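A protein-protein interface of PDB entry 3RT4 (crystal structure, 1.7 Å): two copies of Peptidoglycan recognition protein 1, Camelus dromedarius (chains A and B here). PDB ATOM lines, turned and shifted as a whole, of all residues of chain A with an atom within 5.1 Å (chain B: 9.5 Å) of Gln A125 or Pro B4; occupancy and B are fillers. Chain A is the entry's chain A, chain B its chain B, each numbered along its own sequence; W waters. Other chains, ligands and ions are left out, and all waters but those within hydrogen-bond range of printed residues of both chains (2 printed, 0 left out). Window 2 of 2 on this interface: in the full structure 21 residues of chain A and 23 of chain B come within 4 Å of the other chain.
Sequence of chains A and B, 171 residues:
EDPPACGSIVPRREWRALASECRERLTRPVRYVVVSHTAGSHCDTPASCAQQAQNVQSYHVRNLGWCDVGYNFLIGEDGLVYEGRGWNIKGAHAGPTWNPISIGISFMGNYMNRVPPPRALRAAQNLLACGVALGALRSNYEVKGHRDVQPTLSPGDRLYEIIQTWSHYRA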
ATOM      1  N   LEU A 121     -20.586  13.534   3.396  1.00  0.00           N
ATOM      2  CA  LEU A 121     -19.945  14.227   2.294  1.00  0.00           C
ATOM      3  C   LEU A 121     -19.632  15.657   2.702  1.00  0.00           C
ATOM      4  O   LEU A 121     -18.552  16.154   2.390  1.00  0.00           O
ATOM      5  CB  LEU A 121     -20.822  14.187   1.031  1.00  0.00           C
ATOM      6  CG  LEU A 121     -21.189  12.758   0.560  1.00  0.00           C
ATOM      7  CD1 LEU A 121     -22.331  12.874  -0.439  1.00  0.00           C
ATOM      8  CD2 LEU A 121     -19.978  12.014  -0.047  1.00  0.00           C
ATOM      9  N   ARG A 122     -20.550  16.322   3.403  1.00  0.00           N
ATOM     10  CA  ARG A 122     -20.286  17.684   3.860  1.00  0.00           C
ATOM     11  C   ARG A 122     -19.119  17.739   4.814  1.00  0.00           C
ATOM     12  O   ARG A 122     -18.314  18.655   4.730  1.00  0.00           O
ATOM     13  CB  ARG A 122     -21.463  18.283   4.613  1.00  0.00           C
ATOM     14  CG  ARG A 122     -22.529  18.828   3.737  1.00  0.00           C
ATOM     15  CD  ARG A 122     -23.611  19.480   4.563  1.00  0.00           C
ATOM     16  NE  ARG A 122     -24.202  18.674   5.637  1.00  0.00           N
ATOM     17  CZ  ARG A 122     -25.330  17.985   5.509  1.00  0.00           C
ATOM     18  NH1 ARG A 122     -25.814  17.274   6.516  1.00  0.00           N
ATOM     19  NH2 ARG A 122     -25.942  17.951   4.335  1.00  0.00           N
ATOM     20  N   ALA A 123     -19.018  16.775   5.723  1.00  0.00           N
ATOM     21  CA  ALA A 123     -17.943  16.783   6.709  1.00  0.00           C
ATOM     22  C   ALA A 123     -16.601  16.669   6.015  1.00  0.00           C
ATOM     23  O   ALA A 123     -15.648  17.385   6.340  1.00  0.00           O
ATOM     24  CB  ALA A 123     -18.134  15.635   7.698  1.00  0.00           C
ATOM     25  N   ALA A 124     -16.551  15.768   5.047  1.00  0.00           N
ATOM     26  CA  ALA A 124     -15.352  15.517   4.276  1.00  0.00           C
ATOM     27  C   ALA A 124     -14.850  16.759   3.559  1.00  0.00           C
ATOM     28  O   ALA A 124     -13.674  17.109   3.652  1.00  0.00           O
ATOM     29  CB  ALA A 124     -15.630  14.431   3.259  1.00  0.00           C
ATOM     30  N   GLN A 125     -15.738  17.388   2.797  1.00  0.00           N
ATOM     31  CA  GLN A 125     -15.379  18.579   2.053  1.00  0.00           C
ATOM     32  C   GLN A 125     -15.059  19.723   2.977  1.00  0.00           C
ATOM     33  O   GLN A 125     -14.162  20.513   2.697  1.00  0.00           O
ATOM     34  CB  GLN A 125     -16.510  18.950   1.132  1.00  0.00           C
ATOM     35  CG  GLN A 125     -16.704  17.881   0.123  1.00  0.00           C
ATOM     36  CD  GLN A 125     -17.890  18.132  -0.745  1.00  0.00           C
ATOM     37  OE1 GLN A 125     -19.022  17.879  -0.356  1.00  0.00           O
ATOM     38  NE2 GLN A 125     -17.638  18.636  -1.940  1.00  0.00           N
ATOM     39  N   ASN A 126     -15.801  19.845   4.066  1.00  0.00           N
ATOM     40  CA  ASN A 126     -15.509  20.913   5.006  1.00  0.00           C
ATOM     41  C   ASN A 126     -14.130  20.665   5.641  1.00  0.00           C
ATOM     42  O   ASN A 126     -13.408  21.608   5.940  1.00  0.00           O
ATOM     43  CB  ASN A 126     -16.588  20.982   6.073  1.00  0.00           C
ATOM     44  CG  ASN A 126     -17.869  21.634   5.574  1.00  0.00           C
ATOM     45  OD1 ASN A 126     -18.139  21.669   4.374  1.00  0.00           O
ATOM     46  ND2 ASN A 126     -18.669  22.147   6.500  1.00  0.00           N
ATOM     47  N   LEU A 127     -13.767  19.400   5.846  1.00  0.00           N
ATOM     48  CA  LEU A 127     -12.462  19.076   6.404  1.00  0.00           C
ATOM     49  C   LEU A 127     -11.359  19.577   5.441  1.00  0.00           C
ATOM     50  O   LEU A 127     -10.375  20.190   5.879  1.00  0.00           O
ATOM     51  CB  LEU A 127     -12.343  17.563   6.603  1.00  0.00           C
ATOM     52  CG  LEU A 127     -10.911  17.060   6.865  1.00  0.00           C
ATOM     53  CD1 LEU A 127     -10.426  17.454   8.281  1.00  0.00           C
ATOM     54  CD2 LEU A 127     -10.883  15.552   6.660  1.00  0.00           C
ATOM     55  N   LEU A 128     -11.542  19.357   4.139  1.00  0.00           N
ATOM     56  CA  LEU A 128     -10.555  19.781   3.157  1.00  0.00           C
ATOM     57  C   LEU A 128     -10.416  21.296   3.159  1.00  0.00           C
ATOM     58  O   LEU A 128      -9.292  21.808   3.185  1.00  0.00           O
ATOM     59  CB  LEU A 128     -10.914  19.230   1.779  1.00  0.00           C
ATOM     60  CG  LEU A 128     -11.033  17.710   1.857  1.00  0.00           C
ATOM     61  CD1 LEU A 128     -11.216  17.224   0.449  1.00  0.00           C
ATOM     62  CD2 LEU A 128      -9.814  17.035   2.534  1.00  0.00           C
ATOM     63  N   ALA A 129     -11.543  22.012   3.155  1.00  0.00           N
ATOM     64  CA  ALA A 129     -11.499  23.469   3.199  1.00  0.00           C
ATOM     65  C   ALA A 129     -10.704  23.899   4.448  1.00  0.00           C
ATOM     66  O   ALA A 129      -9.911  24.834   4.355  1.00  0.00           O
ATOM     67  CB  ALA A 129     -12.916  24.071   3.220  1.00  0.00           C
ATOM     68  N   TRP A 166     -16.623  16.611  -7.246  1.00  0.00           N
ATOM     69  CA  TRP A 166     -16.086  17.658  -6.389  1.00  0.00           C
ATOM     70  C   TRP A 166     -15.191  18.641  -7.112  1.00  0.00           C
ATOM     71  O   TRP A 166     -14.473  18.308  -8.055  1.00  0.00           O
ATOM     72  CB  TRP A 166     -15.312  17.085  -5.205  1.00  0.00           C
ATOM     73  CG  TRP A 166     -16.173  16.346  -4.240  1.00  0.00           C
ATOM     74  CD1 TRP A 166     -17.527  16.128  -4.326  1.00  0.00           C
ATOM     75  CD2 TRP A 166     -15.740  15.702  -3.050  1.00  0.00           C
ATOM     76  NE1 TRP A 166     -17.956  15.387  -3.248  1.00  0.00           N
ATOM     77  CE2 TRP A 166     -16.877  15.120  -2.444  1.00  0.00           C
ATOM     78  CE3 TRP A 166     -14.501  15.573  -2.425  1.00  0.00           C
ATOM     79  CZ2 TRP A 166     -16.796  14.397  -1.249  1.00  0.00           C
ATOM     80  CZ3 TRP A 166     -14.420  14.869  -1.245  1.00  0.00           C
ATOM     81  CH2 TRP A 166     -15.559  14.295  -0.660  1.00  0.00           C
ATOM     82  N   GLU B   1     -19.744  19.772  -8.669  1.00  0.00           N
ATOM     83  CA  GLU B   1     -20.204  21.080  -9.215  1.00  0.00           C
ATOM     84  C   GLU B   1     -19.753  22.292  -8.354  1.00  0.00           C
ATOM     85  O   GLU B   1     -18.819  22.992  -8.745  1.00  0.00           O
ATOM     86  CB  GLU B   1     -21.736  21.064  -9.370  1.00  0.00           C
ATOM     87  CG  GLU B   1     -22.273  21.816 -10.604  1.00  0.00           C
ATOM     88  CD  GLU B   1     -22.079  21.053 -11.913  1.00  0.00           C
ATOM     89  OE1 GLU B   1     -22.535  19.890 -11.999  1.00  0.00           O
ATOM     90  OE2 GLU B   1     -21.478  21.618 -12.857  1.00  0.00           O
ATOM     91  N   ASP B   2     -20.397  22.530  -7.201  1.00  0.00           N
ATOM     92  CA  ASP B   2     -20.048  23.643  -6.316  1.00  0.00           C
ATOM     93  C   ASP B   2     -19.888  23.184  -4.861  1.00  0.00           C
ATOM     94  O   ASP B   2     -20.662  22.355  -4.376  1.00  0.00           O
ATOM     95  CB  ASP B   2     -21.137  24.760  -6.442  1.00  0.00           C
ATOM     96  CG  ASP B   2     -22.530  24.206  -6.700  1.00  0.00           C
ATOM     97  OD1 ASP B   2     -23.364  24.250  -5.771  1.00  0.00           O
ATOM     98  OD2 ASP B   2     -22.800  23.735  -7.828  1.00  0.00           O
ATOM     99  N   PRO B   3     -18.902  23.760  -4.128  1.00  0.00           N
ATOM    100  CA  PRO B   3     -18.670  23.324  -2.742  1.00  0.00           C
ATOM    101  C   PRO B   3     -19.683  23.606  -1.630  1.00  0.00           C
ATOM    102  O   PRO B   3     -20.181  24.710  -1.543  1.00  0.00           O
ATOM    103  CB  PRO B   3     -17.306  23.901  -2.435  1.00  0.00           C
ATOM    104  CG  PRO B   3     -17.313  25.249  -3.158  1.00  0.00           C
ATOM    105  CD  PRO B   3     -18.282  25.080  -4.353  1.00  0.00           C
ATOM    106  N   PRO B   4     -19.997  22.578  -0.779  1.00  0.00           N
ATOM    107  CA  PRO B   4     -20.947  22.805   0.324  1.00  0.00           C
ATOM    108  C   PRO B   4     -20.250  23.791   1.262  1.00  0.00           C
ATOM    109  O   PRO B   4     -19.081  23.582   1.632  1.00  0.00           O
ATOM    110  CB  PRO B   4     -21.070  21.436   0.996  1.00  0.00           C
ATOM    111  CG  PRO B   4     -20.753  20.477  -0.064  1.00  0.00           C
ATOM    112  CD  PRO B   4     -19.659  21.145  -0.887  1.00  0.00           C
ATOM    113  N   ALA B   5     -20.964  24.840   1.667  1.00  0.00           N
ATOM    114  CA  ALA B   5     -20.414  25.870   2.545  1.00  0.00           C
ATOM    115  C   ALA B   5     -19.980  25.329   3.900  1.00  0.00           C
ATOM    116  O   ALA B   5     -20.428  24.269   4.339  1.00  0.00           O
ATOM    117  CB  ALA B   5     -21.425  27.013   2.718  1.00  0.00           C
ATOM    118  N   CYS B   6     -19.099  26.067   4.553  1.00  0.00           N
ATOM    119  CA  CYS B   6     -18.559  25.672   5.839  1.00  0.00           C
ATOM    120  C   CYS B   6     -19.579  25.369   6.927  1.00  0.00           C
ATOM    121  O   CYS B   6     -20.769  25.662   6.792  1.00  0.00           O
ATOM    122  CB  CYS B   6     -17.634  26.767   6.320  1.00  0.00           C
ATOM    123  SG  CYS B   6     -18.356  28.441   6.278  1.00  0.00           S
ATOM    124  N   GLY B   7     -19.079  24.753   7.992  1.00  0.00           N
ATOM    125  CA  GLY B   7     -19.900  24.438   9.142  1.00  0.00           C
ATOM    126  C   GLY B   7     -20.649  23.123   9.195  1.00  0.00           C
ATOM    127  O   GLY B   7     -21.283  22.846  10.207  1.00  0.00           O
ATOM    128  N   SER B   8     -20.570  22.320   8.131  1.00  0.00           N
ATOM    129  CA  SER B   8     -21.245  21.003   8.023  1.00  0.00           C
ATOM    130  C   SER B   8     -22.638  21.086   8.626  1.00  0.00           C
ATOM    131  O   SER B   8     -23.038  20.280   9.473  1.00  0.00           O
ATOM    132  CB  SER B   8     -20.459  19.932   8.771  1.00  0.00           C
ATOM    133  OG  SER B   8     -19.072  20.075   8.541  1.00  0.00           O
ATOM    134  N   ILE B   9     -23.385  22.051   8.145  1.00  0.00           N
ATOM    135  CA  ILE B   9     -24.700  22.306   8.655  1.00  0.00           C
ATOM    136  C   ILE B   9     -25.706  21.402   7.990  1.00  0.00           C
ATOM    137  O   ILE B   9     -25.648  21.171   6.788  1.00  0.00           O
ATOM    138  CB  ILE B   9     -25.045  23.838   8.417  1.00  0.00           C
ATOM    139  CG1 ILE B   9     -24.033  24.725   9.163  1.00  0.00           C
ATOM    140  CG2 ILE B   9     -26.470  24.189   8.863  1.00  0.00           C
ATOM    141  CD1 ILE B   9     -24.060  26.163   8.671  1.00  0.00           C
ATOM    142  N   PRO B  11     -28.849  20.952   6.343  1.00  0.00           N
ATOM    143  CA  PRO B  11     -29.809  21.875   5.713  1.00  0.00           C
ATOM    144  C   PRO B  11     -31.236  21.679   6.180  1.00  0.00           C
ATOM    145  O   PRO B  11     -31.654  20.560   6.507  1.00  0.00           O
ATOM    146  CB  PRO B  11     -29.710  21.583   4.225  1.00  0.00           C
ATOM    147  CG  PRO B  11     -28.649  20.537   4.053  1.00  0.00           C
ATOM    148  CD  PRO B  11     -28.221  20.023   5.392  1.00  0.00           C
ATOM    149  N   ASN B 126     -17.161  25.516  15.272  1.00  0.00           N
ATOM    150  CA  ASN B 126     -17.014  25.302  13.822  1.00  0.00           C
ATOM    151  C   ASN B 126     -17.990  26.271  13.128  1.00  0.00           C
ATOM    152  O   ASN B 126     -17.639  26.961  12.167  1.00  0.00           O
ATOM    153  CB  ASN B 126     -17.387  23.808  13.504  1.00  0.00           C
ATOM    154  CG  ASN B 126     -17.527  23.457  11.966  1.00  0.00           C
ATOM    155  OD1 ASN B 126     -17.465  24.316  11.078  1.00  0.00           O
ATOM    156  ND2 ASN B 126     -17.736  22.158  11.686  1.00  0.00           N
ATOM    157  N   CYS B 130     -17.095  29.450  10.741  1.00  0.00           N
ATOM    158  CA  CYS B 130     -17.682  29.479   9.408  1.00  0.00           C
ATOM    159  C   CYS B 130     -18.428  30.803   9.148  1.00  0.00           C
ATOM    160  O   CYS B 130     -18.355  31.362   8.055  1.00  0.00           O
ATOM    161  CB  CYS B 130     -18.632  28.307   9.253  1.00  0.00           C
ATOM    162  SG  CYS B 130     -19.707  28.403   7.785  1.00  0.00           S
ATOM    163  N   LEU B 134     -17.492  33.442   6.189  1.00  0.00           N
ATOM    164  CA  LEU B 134     -18.551  33.809   5.284  1.00  0.00           C
ATOM    165  C   LEU B 134     -18.774  35.303   5.185  1.00  0.00           C
ATOM    166  O   LEU B 134     -19.294  35.776   4.185  1.00  0.00           O
ATOM    167  CB  LEU B 134     -19.865  33.189   5.744  1.00  0.00           C
ATOM    168  CG  LEU B 134     -20.318  31.924   5.010  1.00  0.00           C
ATOM    169  CD1 LEU B 134     -21.450  31.187   5.758  1.00  0.00           C
ATOM    170  CD2 LEU B 134     -20.758  32.352   3.614  1.00  0.00           C
HETATM  171  O   HOH W   1     -19.632  19.268  -4.610  1.00  0.00           O
HETATM  172  O   HOH W   2     -24.202  17.884   8.631  1.00  0.00           O
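The backbone carbonyl oxygen (O) of Ile B9 lies within hydrogen-bond range of the guanidinium group (NE) of Arg A122 (3.1 Å). The side-chain amide oxygen (OD1) of Asn A126 sits close to the backbone carbonyl oxygen (O) of Pro B4. The side-chain amide oxygen (OD1) of Asn A126 sits close to the backbone carbonyl oxygen (O) of Ala B5, at 3.5 Å. The side-chain amide nitrogen (ND2) of Asn A126 sits close to the backbone NH (N) of Gly B7 (3.0 Å). ND2 of Asn A126 lies close to N of Ser B8.
OE1 of Gln A125 lies close to O of Leu A121 (3.3 Å). The backbone carbonyl oxygen of Arg A122 lies close to the side-chain amide oxygen of Asn A126 (3.0 Å). The side-chain sulfur (SG) of Cys B130 forms a disulfide with the side-chain sulfur (SG) of Cys B6. The side-chain sulfur (SG) of Cys B130 sits at hydrogen-bond distance from the backbone NH (N) of Gly B7 (3.7 Å).
Pro B11 touches Arg A122 (CD to NH2, 3.3 Å). Ser B8 touches Ala A123 (OG to CA, 3.9 Å). Gln A125 touches Pro B4 (OE1 to CG, 3.1 Å). Asn A126 touches Cys B6.
Gln A125 touches just one residue of chain B: Pro B4 (3.1 Å). Pro B4 touches two residues of chain A. No residue of chain B comes within 4 Å of Ala A124. Asn A126 touches just these residues of chain B: Pro B4, Ala B5, Cys B6, Gly B7 and Ser B8. Of the printed residues of chain A, Ser B8 touches Ala A123 and Asn A126. Of the printed residues of chain A, Ile B9 touches Arg A122 (3.1 Å). Leu A127 touches none of the printed residues of chain B. The nearest printed residue of chain A that does not touch Cys B6 is Ala A129 (6.3 Å).
Of the 10 printed residues of chain A, 4 touch a printed residue of chain B. Hydrophobic or aromatic side chains of chain B that line the printed part of chain A: Pro B4 and Pro B11. Among the printed residues, 9 pairs touch across the chains.
Position printed for both chains: 126. Of the 9 pairs that touch across the chains among the printed residues, none has its exchanged pair printed and touching as well.
Water W2 bridges NH1 of Arg A122 (2.7 Å) and O of Ser B8 (2.8 Å). Water W1 bridges the backbone carbonyl oxygen of Asp B2 (3.3 Å) and the side-chain amide nitrogen of Gln A125 (3.4 Å).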
